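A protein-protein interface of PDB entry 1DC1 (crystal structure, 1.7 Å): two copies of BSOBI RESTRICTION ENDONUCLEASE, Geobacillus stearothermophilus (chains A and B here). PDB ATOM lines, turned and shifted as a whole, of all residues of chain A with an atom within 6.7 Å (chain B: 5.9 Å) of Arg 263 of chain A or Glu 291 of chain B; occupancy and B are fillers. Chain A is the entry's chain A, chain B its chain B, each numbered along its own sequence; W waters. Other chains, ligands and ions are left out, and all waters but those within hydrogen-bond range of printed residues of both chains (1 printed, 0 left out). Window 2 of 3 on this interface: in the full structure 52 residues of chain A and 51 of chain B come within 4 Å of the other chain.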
ATOM      1  N   LEU A 206      -9.772 -30.284   6.618  1.00  0.00           N
ATOM      2  CA  LEU A 206     -10.928 -30.618   5.788  1.00  0.00           C
ATOM      3  C   LEU A 206     -11.098 -29.735   4.578  1.00  0.00           C
ATOM      4  O   LEU A 206     -11.446 -30.227   3.499  1.00  0.00           O
ATOM      5  CB  LEU A 206     -12.229 -30.586   6.588  1.00  0.00           C
ATOM      6  CG  LEU A 206     -12.697 -31.823   7.346  1.00  0.00           C
ATOM      7  CD1 LEU A 206     -14.110 -31.547   7.886  1.00  0.00           C
ATOM      8  CD2 LEU A 206     -12.656 -33.057   6.446  1.00  0.00           C
ATOM      9  N   VAL A 207     -10.882 -28.426   4.745  1.00  0.00           N
ATOM     10  CA  VAL A 207     -10.967 -27.494   3.612  1.00  0.00           C
ATOM     11  C   VAL A 207      -9.647 -27.464   2.837  1.00  0.00           C
ATOM     12  O   VAL A 207      -9.665 -27.064   1.687  1.00  0.00           O
ATOM     13  CB  VAL A 207     -11.182 -26.000   4.020  1.00  0.00           C
ATOM     14  CG1 VAL A 207     -12.464 -25.513   3.502  1.00  0.00           C
ATOM     15  CG2 VAL A 207     -11.040 -25.821   5.501  1.00  0.00           C
ATOM     16  N   LYS A 209      -7.174 -25.465   3.396  1.00  0.00           N
ATOM     17  CA  LYS A 209      -6.930 -24.046   3.228  1.00  0.00           C
ATOM     18  C   LYS A 209      -6.520 -23.498   4.577  1.00  0.00           C
ATOM     19  O   LYS A 209      -6.830 -24.045   5.629  1.00  0.00           O
ATOM     20  CB  LYS A 209      -8.198 -23.312   2.777  1.00  0.00           C
ATOM     21  CG  LYS A 209      -8.722 -23.704   1.388  1.00  0.00           C
ATOM     22  CD  LYS A 209      -7.898 -23.089   0.249  1.00  0.00           C
ATOM     23  CE  LYS A 209      -8.177 -23.732  -1.114  1.00  0.00           C
ATOM     24  NZ  LYS A 209      -7.904 -25.177  -1.032  1.00  0.00           N
ATOM     25  N   ASN A 258     -15.483 -14.208   2.006  1.00  0.00           N
ATOM     26  CA  ASN A 258     -16.738 -14.881   1.902  1.00  0.00           C
ATOM     27  C   ASN A 258     -16.615 -16.247   1.217  1.00  0.00           C
ATOM     28  O   ASN A 258     -17.286 -17.191   1.626  1.00  0.00           O
ATOM     29  CB  ASN A 258     -17.728 -13.998   1.171  1.00  0.00           C
ATOM     30  CG  ASN A 258     -19.068 -14.626   1.104  1.00  0.00           C
ATOM     31  OD1 ASN A 258     -19.757 -14.716   2.117  1.00  0.00           O
ATOM     32  ND2 ASN A 258     -19.444 -15.104  -0.073  1.00  0.00           N
ATOM     33  N   THR A 259     -15.779 -16.358   0.172  1.00  0.00           N
ATOM     34  CA  THR A 259     -15.566 -17.644  -0.458  1.00  0.00           C
ATOM     35  C   THR A 259     -14.810 -18.549   0.523  1.00  0.00           C
ATOM     36  O   THR A 259     -15.146 -19.752   0.639  1.00  0.00           O
ATOM     37  CB  THR A 259     -14.799 -17.522  -1.739  1.00  0.00           C
ATOM     38  OG1 THR A 259     -15.644 -16.880  -2.697  1.00  0.00           O
ATOM     39  CG2 THR A 259     -14.437 -18.860  -2.288  1.00  0.00           C
ATOM     40  N   ALA A 260     -13.802 -18.001   1.224  1.00  0.00           N
ATOM     41  CA  ALA A 260     -13.086 -18.784   2.233  1.00  0.00           C
ATOM     42  C   ALA A 260     -14.096 -19.363   3.261  1.00  0.00           C
ATOM     43  O   ALA A 260     -14.056 -20.546   3.570  1.00  0.00           O
ATOM     44  CB  ALA A 260     -12.080 -17.929   2.953  1.00  0.00           C
ATOM     45  N   LEU A 261     -15.003 -18.532   3.784  1.00  0.00           N
ATOM     46  CA  LEU A 261     -15.969 -18.992   4.789  1.00  0.00           C
ATOM     47  C   LEU A 261     -16.972 -20.031   4.224  1.00  0.00           C
ATOM     48  O   LEU A 261     -17.415 -20.960   4.927  1.00  0.00           O
ATOM     49  CB  LEU A 261     -16.724 -17.788   5.406  1.00  0.00           C
ATOM     50  CG  LEU A 261     -15.922 -16.904   6.372  1.00  0.00           C
ATOM     51  CD1 LEU A 261     -16.787 -15.699   6.743  1.00  0.00           C
ATOM     52  CD2 LEU A 261     -15.480 -17.652   7.626  1.00  0.00           C
ATOM     53  N   THR A 262     -17.325 -19.864   2.955  1.00  0.00           N
ATOM     54  CA  THR A 262     -18.205 -20.793   2.282  1.00  0.00           C
ATOM     55  C   THR A 262     -17.485 -22.161   2.101  1.00  0.00           C
ATOM     56  O   THR A 262     -18.062 -23.226   2.323  1.00  0.00           O
ATOM     57  CB  THR A 262     -18.614 -20.239   0.910  1.00  0.00           C
ATOM     58  OG1 THR A 262     -19.324 -19.009   1.087  1.00  0.00           O
ATOM     59  CG2 THR A 262     -19.482 -21.229   0.189  1.00  0.00           C
ATOM     60  N   ARG A 263     -16.229 -22.147   1.677  1.00  0.00           N
ATOM     61  CA  ARG A 263     -15.525 -23.405   1.566  1.00  0.00           C
ATOM     62  C   ARG A 263     -15.567 -24.116   2.933  1.00  0.00           C
ATOM     63  O   ARG A 263     -15.781 -25.315   2.998  1.00  0.00           O
ATOM     64  CB  ARG A 263     -14.063 -23.173   1.136  1.00  0.00           C
ATOM     65  CG  ARG A 263     -13.900 -22.603  -0.277  1.00  0.00           C
ATOM     66  CD  ARG A 263     -12.427 -22.248  -0.520  1.00  0.00           C
ATOM     67  NE  ARG A 263     -12.078 -22.212  -1.936  1.00  0.00           N
ATOM     68  CZ  ARG A 263     -10.945 -21.683  -2.404  1.00  0.00           C
ATOM     69  NH1 ARG A 263     -10.074 -21.155  -1.565  1.00  0.00           N
ATOM     70  NH2 ARG A 263     -10.667 -21.692  -3.707  1.00  0.00           N
ATOM     71  N   ILE A 264     -15.360 -23.361   4.015  1.00  0.00           N
ATOM     72  CA  ILE A 264     -15.351 -23.896   5.384  1.00  0.00           C
ATOM     73  C   ILE A 264     -16.675 -24.534   5.763  1.00  0.00           C
ATOM     74  O   ILE A 264     -16.720 -25.691   6.198  1.00  0.00           O
ATOM     75  CB  ILE A 264     -15.025 -22.769   6.417  1.00  0.00           C
ATOM     76  CG1 ILE A 264     -13.520 -22.426   6.325  1.00  0.00           C
ATOM     77  CG2 ILE A 264     -15.473 -23.213   7.818  1.00  0.00           C
ATOM     78  CD1 ILE A 264     -13.081 -21.168   7.069  1.00  0.00           C
ATOM     79  N   ARG A 265     -17.745 -23.771   5.586  1.00  0.00           N
ATOM     80  CA  ARG A 265     -19.094 -24.232   5.899  1.00  0.00           C
ATOM     81  C   ARG A 265     -19.430 -25.461   5.095  1.00  0.00           C
ATOM     82  O   ARG A 265     -20.025 -26.426   5.605  1.00  0.00           O
ATOM     83  CB  ARG A 265     -20.125 -23.183   5.525  1.00  0.00           C
ATOM     84  CG  ARG A 265     -20.229 -22.128   6.518  1.00  0.00           C
ATOM     85  CD  ARG A 265     -21.214 -21.075   6.119  1.00  0.00           C
ATOM     86  NE  ARG A 265     -20.869 -19.877   6.865  1.00  0.00           N
ATOM     87  CZ  ARG A 265     -20.511 -18.720   6.319  1.00  0.00           C
ATOM     88  NH1 ARG A 265     -20.457 -18.596   4.994  1.00  0.00           N
ATOM     89  NH2 ARG A 265     -20.142 -17.715   7.113  1.00  0.00           N
ATOM     90  N   ASN A 266     -19.088 -25.401   3.815  1.00  0.00           N
ATOM     91  CA  ASN A 266     -19.359 -26.510   2.899  1.00  0.00           C
ATOM     92  C   ASN A 266     -18.662 -27.818   3.309  1.00  0.00           C
ATOM     93  O   ASN A 266     -19.317 -28.847   3.495  1.00  0.00           O
ATOM     94  CB  ASN A 266     -18.947 -26.143   1.477  1.00  0.00           C
ATOM     95  CG  ASN A 266     -20.010 -25.290   0.743  1.00  0.00           C
ATOM     96  OD1 ASN A 266     -21.062 -24.980   1.295  1.00  0.00           O
ATOM     97  ND2 ASN A 266     -19.713 -24.909  -0.495  1.00  0.00           N
ATOM     98  N   LYS A 267     -17.341 -27.780   3.437  1.00  0.00           N
ATOM     99  CA  LYS A 267     -16.574 -28.959   3.845  1.00  0.00           C
ATOM    100  C   LYS A 267     -16.935 -29.483   5.211  1.00  0.00           C
ATOM    101  O   LYS A 267     -17.049 -30.693   5.386  1.00  0.00           O
ATOM    102  CB  LYS A 267     -15.064 -28.698   3.800  1.00  0.00           C
ATOM    103  CG  LYS A 267     -14.627 -28.000   2.572  1.00  0.00           C
ATOM    104  CD  LYS A 267     -13.946 -28.980   1.712  1.00  0.00           C
ATOM    105  CE  LYS A 267     -14.885 -29.462   0.642  1.00  0.00           C
ATOM    106  NZ  LYS A 267     -14.372 -30.737   0.082  1.00  0.00           N
ATOM    107  N   PHE A 268     -17.116 -28.609   6.196  1.00  0.00           N
ATOM    108  CA  PHE A 268     -17.490 -29.102   7.503  1.00  0.00           C
ATOM    109  C   PHE A 268     -18.907 -29.705   7.537  1.00  0.00           C
ATOM    110  O   PHE A 268     -19.065 -30.790   8.077  1.00  0.00           O
ATOM    111  CB  PHE A 268     -17.275 -28.011   8.541  1.00  0.00           C
ATOM    112  CG  PHE A 268     -15.830 -27.906   8.994  1.00  0.00           C
ATOM    113  CD1 PHE A 268     -14.851 -27.404   8.122  1.00  0.00           C
ATOM    114  CD2 PHE A 268     -15.424 -28.394  10.259  1.00  0.00           C
ATOM    115  CE1 PHE A 268     -13.479 -27.405   8.502  1.00  0.00           C
ATOM    116  CE2 PHE A 268     -14.055 -28.396  10.644  1.00  0.00           C
ATOM    117  CZ  PHE A 268     -13.095 -27.910   9.772  1.00  0.00           C
ATOM    118  N   GLU A 270     -20.508 -31.206   5.324  1.00  0.00           N
ATOM    119  CA  GLU A 270     -20.403 -32.491   4.648  1.00  0.00           C
ATOM    120  C   GLU A 270     -20.122 -33.551   5.668  1.00  0.00           C
ATOM    121  O   GLU A 270     -20.510 -34.696   5.519  1.00  0.00           O
ATOM    122  CB  GLU A 270     -19.202 -32.547   3.705  1.00  0.00           C
ATOM    123  CG  GLU A 270     -19.321 -31.847   2.383  1.00  0.00           C
ATOM    124  CD  GLU A 270     -17.964 -31.761   1.632  1.00  0.00           C
ATOM    125  OE1 GLU A 270     -17.041 -32.614   1.858  1.00  0.00           O
ATOM    126  OE2 GLU A 270     -17.844 -30.814   0.809  1.00  0.00           O
ATOM    127  N   ASP B 251      -5.587 -18.315  -6.616  1.00  0.00           N
ATOM    128  CA  ASP B 251      -6.690 -18.677  -5.729  1.00  0.00           C
ATOM    129  C   ASP B 251      -7.301 -17.421  -5.055  1.00  0.00           C
ATOM    130  O   ASP B 251      -8.536 -17.350  -4.842  1.00  0.00           O
ATOM    131  CB  ASP B 251      -6.212 -19.651  -4.660  1.00  0.00           C
ATOM    132  CG  ASP B 251      -7.374 -20.345  -3.990  1.00  0.00           C
ATOM    133  OD1 ASP B 251      -7.919 -21.284  -4.637  1.00  0.00           O
ATOM    134  OD2 ASP B 251      -7.746 -19.913  -2.870  1.00  0.00           O
ATOM    135  N   TRP B 254      -9.572 -15.750  -7.538  1.00  0.00           N
ATOM    136  CA  TRP B 254     -10.640 -16.675  -7.894  1.00  0.00           C
ATOM    137  C   TRP B 254     -11.669 -16.620  -6.712  1.00  0.00           C
ATOM    138  O   TRP B 254     -12.867 -16.577  -6.961  1.00  0.00           O
ATOM    139  CB  TRP B 254     -10.096 -18.098  -8.067  1.00  0.00           C
ATOM    140  CG  TRP B 254     -11.157 -19.153  -7.856  1.00  0.00           C
ATOM    141  CD1 TRP B 254     -11.172 -20.099  -6.883  1.00  0.00           C
ATOM    142  CD2 TRP B 254     -12.365 -19.356  -8.639  1.00  0.00           C
ATOM    143  NE1 TRP B 254     -12.299 -20.888  -7.005  1.00  0.00           N
ATOM    144  CE2 TRP B 254     -13.050 -20.455  -8.069  1.00  0.00           C
ATOM    145  CE3 TRP B 254     -12.934 -18.712  -9.764  1.00  0.00           C
ATOM    146  CZ2 TRP B 254     -14.285 -20.936  -8.583  1.00  0.00           C
ATOM    147  CZ3 TRP B 254     -14.173 -19.201 -10.286  1.00  0.00           C
ATOM    148  CH2 TRP B 254     -14.826 -20.305  -9.686  1.00  0.00           C
ATOM    149  N   LYS B 255     -11.210 -16.617  -5.440  1.00  0.00           N
ATOM    150  CA  LYS B 255     -12.126 -16.531  -4.276  1.00  0.00           C
ATOM    151  C   LYS B 255     -12.968 -15.250  -4.433  1.00  0.00           C
ATOM    152  O   LYS B 255     -14.164 -15.240  -4.204  1.00  0.00           O
ATOM    153  CB  LYS B 255     -11.334 -16.447  -2.974  1.00  0.00           C
ATOM    154  CG  LYS B 255     -10.880 -17.792  -2.442  1.00  0.00           C
ATOM    155  CD  LYS B 255     -10.204 -17.646  -1.066  1.00  0.00           C
ATOM    156  CE  LYS B 255      -8.879 -16.905  -1.105  1.00  0.00           C
ATOM    157  NZ  LYS B 255      -7.760 -17.863  -1.172  1.00  0.00           N
ATOM    158  N   HIS B 286      -4.318 -25.874  -9.309  1.00  0.00           N
ATOM    159  CA  HIS B 286      -5.095 -27.090  -9.184  1.00  0.00           C
ATOM    160  C   HIS B 286      -6.385 -27.053  -8.342  1.00  0.00           C
ATOM    161  O   HIS B 286      -7.458 -27.466  -8.807  1.00  0.00           O
ATOM    162  CB  HIS B 286      -4.235 -28.213  -8.663  1.00  0.00           C
ATOM    163  CG  HIS B 286      -5.009 -29.463  -8.552  1.00  0.00           C
ATOM    164  ND1 HIS B 286      -5.553 -30.076  -9.661  1.00  0.00           N
ATOM    165  CD2 HIS B 286      -5.531 -30.095  -7.481  1.00  0.00           C
ATOM    166  CE1 HIS B 286      -6.378 -31.031  -9.280  1.00  0.00           C
ATOM    167  NE2 HIS B 286      -6.387 -31.065  -7.960  1.00  0.00           N
ATOM    168  N   SER B 287      -6.303 -26.551  -7.109  1.00  0.00           N
ATOM    169  CA  SER B 287      -7.483 -26.492  -6.232  1.00  0.00           C
ATOM    170  C   SER B 287      -8.630 -25.725  -6.845  1.00  0.00           C
ATOM    171  O   SER B 287      -9.784 -26.246  -6.912  1.00  0.00           O
ATOM    172  CB  SER B 287      -7.165 -25.829  -4.921  1.00  0.00           C
ATOM    173  OG  SER B 287      -8.322 -25.800  -4.129  1.00  0.00           O
ATOM    174  N   MET B 288      -8.350 -24.483  -7.263  1.00  0.00           N
ATOM    175  CA  MET B 288      -9.386 -23.683  -7.929  1.00  0.00           C
ATOM    176  C   MET B 288      -9.896 -24.349  -9.256  1.00  0.00           C
ATOM    177  O   MET B 288     -11.081 -24.235  -9.602  1.00  0.00           O
ATOM    178  CB  MET B 288      -8.877 -22.261  -8.173  1.00  0.00           C
ATOM    179  CG  MET B 288      -7.677 -22.123  -9.097  1.00  0.00           C
ATOM    180  SD  MET B 288      -7.278 -20.389  -9.299  1.00  0.00           S
ATOM    181  CE  MET B 288      -8.365 -19.826 -10.585  1.00  0.00           C
ATOM    182  N   ALA B 289      -9.023 -25.042  -9.980  1.00  0.00           N
ATOM    183  CA  ALA B 289      -9.411 -25.738 -11.205  1.00  0.00           C
ATOM    184  C   ALA B 289     -10.454 -26.781 -10.854  1.00  0.00           C
ATOM    185  O   ALA B 289     -11.415 -26.957 -11.598  1.00  0.00           O
ATOM    186  CB  ALA B 289      -8.195 -26.419 -11.891  1.00  0.00           C
ATOM    187  N   GLU B 290     -10.276 -27.466  -9.724  1.00  0.00           N
ATOM    188  CA  GLU B 290     -11.238 -28.469  -9.290  1.00  0.00           C
ATOM    189  C   GLU B 290     -12.585 -27.811  -9.024  1.00  0.00           C
ATOM    190  O   GLU B 290     -13.639 -28.336  -9.402  1.00  0.00           O
ATOM    191  CB  GLU B 290     -10.748 -29.131  -8.029  1.00  0.00           C
ATOM    192  CG  GLU B 290      -9.546 -30.021  -8.259  1.00  0.00           C
ATOM    193  CD  GLU B 290      -9.939 -31.494  -8.452  1.00  0.00           C
ATOM    194  OE1 GLU B 290     -11.093 -31.784  -8.872  1.00  0.00           O
ATOM    195  OE2 GLU B 290      -9.086 -32.368  -8.180  1.00  0.00           O
ATOM    196  N   GLU B 291     -12.564 -26.659  -8.376  1.00  0.00           N
ATOM    197  CA  GLU B 291     -13.818 -25.981  -8.080  1.00  0.00           C
ATOM    198  C   GLU B 291     -14.517 -25.473  -9.350  1.00  0.00           C
ATOM    199  O   GLU B 291     -15.759 -25.517  -9.448  1.00  0.00           O
ATOM    200  CB  GLU B 291     -13.553 -24.814  -7.133  1.00  0.00           C
ATOM    201  CG  GLU B 291     -13.281 -25.285  -5.740  1.00  0.00           C
ATOM    202  CD  GLU B 291     -12.952 -24.146  -4.838  1.00  0.00           C
ATOM    203  OE1 GLU B 291     -12.596 -23.085  -5.389  1.00  0.00           O
ATOM    204  OE2 GLU B 291     -13.034 -24.307  -3.591  1.00  0.00           O
ATOM    205  N   ILE B 292     -13.744 -24.961 -10.310  1.00  0.00           N
ATOM    206  CA  ILE B 292     -14.320 -24.471 -11.576  1.00  0.00           C
ATOM    207  C   ILE B 292     -14.958 -25.652 -12.307  1.00  0.00           C
ATOM    208  O   ILE B 292     -16.079 -25.547 -12.777  1.00  0.00           O
ATOM    209  CB  ILE B 292     -13.260 -23.817 -12.502  1.00  0.00           C
ATOM    210  CG1 ILE B 292     -12.776 -22.511 -11.864  1.00  0.00           C
ATOM    211  CG2 ILE B 292     -13.854 -23.567 -13.942  1.00  0.00           C
ATOM    212  CD1 ILE B 292     -11.460 -22.024 -12.390  1.00  0.00           C
ATOM    213  N   TRP B 293     -14.236 -26.769 -12.379  1.00  0.00           N
ATOM    214  CA  TRP B 293     -14.739 -27.972 -13.016  1.00  0.00           C
ATOM    215  C   TRP B 293     -16.035 -28.441 -12.342  1.00  0.00           C
ATOM    216  O   TRP B 293     -17.025 -28.754 -13.017  1.00  0.00           O
ATOM    217  CB  TRP B 293     -13.682 -29.032 -12.937  1.00  0.00           C
ATOM    218  CG  TRP B 293     -14.077 -30.288 -13.537  1.00  0.00           C
ATOM    219  CD1 TRP B 293     -14.646 -31.346 -12.914  1.00  0.00           C
ATOM    220  CD2 TRP B 293     -13.912 -30.653 -14.893  1.00  0.00           C
ATOM    221  NE1 TRP B 293     -14.847 -32.363 -13.796  1.00  0.00           N
ATOM    222  CE2 TRP B 293     -14.407 -31.968 -15.028  1.00  0.00           C
ATOM    223  CE3 TRP B 293     -13.395 -29.998 -16.020  1.00  0.00           C
ATOM    224  CZ2 TRP B 293     -14.401 -32.650 -16.251  1.00  0.00           C
ATOM    225  CZ3 TRP B 293     -13.387 -30.662 -17.231  1.00  0.00           C
ATOM    226  CH2 TRP B 293     -13.888 -31.979 -17.341  1.00  0.00           C
ATOM    227  N   ASP B 294     -16.057 -28.484 -11.020  1.00  0.00           N
ATOM    228  CA  ASP B 294     -17.270 -28.881 -10.322  1.00  0.00           C
ATOM    229  C   ASP B 294     -18.448 -27.970 -10.686  1.00  0.00           C
ATOM    230  O   ASP B 294     -19.582 -28.429 -10.859  1.00  0.00           O
ATOM    231  CB  ASP B 294     -17.055 -28.830  -8.816  1.00  0.00           C
ATOM    232  CG  ASP B 294     -16.201 -29.968  -8.339  1.00  0.00           C
ATOM    233  OD1 ASP B 294     -15.947 -30.861  -9.186  1.00  0.00           O
ATOM    234  OD2 ASP B 294     -15.788 -29.970  -7.149  1.00  0.00           O
ATOM    235  N   GLN B 295     -18.183 -26.669 -10.766  1.00  0.00           N
ATOM    236  CA  GLN B 295     -19.224 -25.677 -11.110  1.00  0.00           C
ATOM    237  C   GLN B 295     -19.690 -25.823 -12.554  1.00  0.00           C
ATOM    238  O   GLN B 295     -20.863 -25.584 -12.853  1.00  0.00           O
ATOM    239  CB  GLN B 295     -18.711 -24.243 -10.850  1.00  0.00           C
ATOM    240  CG  GLN B 295     -18.570 -23.948  -9.372  1.00  0.00           C
ATOM    241  CD  GLN B 295     -18.369 -22.477  -9.093  1.00  0.00           C
ATOM    242  OE1 GLN B 295     -18.748 -21.653  -9.894  1.00  0.00           O
ATOM    243  NE2 GLN B 295     -17.769 -22.145  -7.955  1.00  0.00           N
ATOM    244  N   LEU B 296     -18.775 -26.181 -13.453  1.00  0.00           N
ATOM    245  CA  LEU B 296     -19.175 -26.404 -14.837  1.00  0.00           C
ATOM    246  C   LEU B 296     -20.064 -27.676 -14.881  1.00  0.00           C
ATOM    247  O   LEU B 296     -21.082 -27.702 -15.551  1.00  0.00           O
ATOM    248  CB  LEU B 296     -17.961 -26.601 -15.758  1.00  0.00           C
ATOM    249  CG  LEU B 296     -17.093 -25.356 -16.050  1.00  0.00           C
ATOM    250  CD1 LEU B 296     -15.755 -25.822 -16.645  1.00  0.00           C
ATOM    251  CD2 LEU B 296     -17.809 -24.326 -16.980  1.00  0.00           C
HETATM  252  O   HOH W   1     -10.636 -25.743  -2.511  1.00  0.00           O
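The side-chain amino group of Lys 209 of chain A is in hydrogen-bond range of the side-chain hydroxyl of Ser 287 of chain B (3.2 Å). NE of Arg 263 of chain A is in salt-bridge range of OE2 of Glu 291 of chain B, at 2.8 Å. The side-chain hydroxyl of Thr 259 of chain A lies within hydrogen-bond range of the backbone carbonyl oxygen of Lys 255 of chain B (2.7 Å). The side-chain carboxylate of Asp 251 of chain B lies within salt-bridge range of the guanidinium group of Arg 263 of chain A (2.9 Å).
NZ of Lys 255 of chain B is in salt-bridge range of OD2 of Asp 251 of chain B. The indole nitrogen of Trp 254 of chain B lies within hydrogen-bond range of the side-chain carboxylate of Glu 291 of chain B. N of Asp 251 of chain B lies within hydrogen-bond range of SD of Met 288 of chain B (3.8 Å).
Trp 254 of chain B touches Arg 263 of chain A (CD1 to NH2, 3.6 Å). CD of Lys 255 of chain B touches NH1 of Arg 263 of chain A (3.5 Å).
Printed residues of chain B within 4 Å of Lys 209 of chain A: Ser 287 (3.2 Å). Of chain B, only Asp 251 (2.9 Å), Trp 254 (3.6 Å), Lys 255 (3.5 Å) and Glu 291 (2.8 Å) come within 4 Å of Arg 263 of chain A. Of the printed residues of chain A, Asp 251 of chain B touches Arg 263. Printed residues of chain A within 4 Å of Trp 254 of chain B: Arg 263. Of the printed residues of chain A, Lys 255 of chain B touches Thr 259 (2.7 Å) and Arg 263 (3.5 Å). Glu 291 of chain B touches just one residue of chain A: Arg 263 (2.8 Å). The nearest printed residue of chain B that does not touch Arg 263 of chain A is Ser 287 of chain B (4.7 Å).
Of the 15 printed residues of chain A, 3 touch a printed residue of chain B. Printed residues of chain B that touch a printed residue of chain A: Asp 251, Trp 254, Lys 255, Ser 287 and Glu 291. Among the printed residues, 6 pairs touch across the chains. Among the printed residues, Asp or Glu carboxylates within 4 Å of a Lys or Arg side-chain nitrogen of the other chain: Arg 263 of chain A with Asp 251 of chain B and Arg 263 of chain A with Glu 291 of chain B.
No position is printed for both chains. Of the 6 pairs that touch across the chains among the printed residues, none has its exchanged pair printed and touching as well.
Water W1 lies within hydrogen-bond range of OG of Ser 287 of chain B (2.8 Å), OE2 of Glu 291 of chain B (3.0 Å) and NZ of Lys 209 of chain A (3.2 Å).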
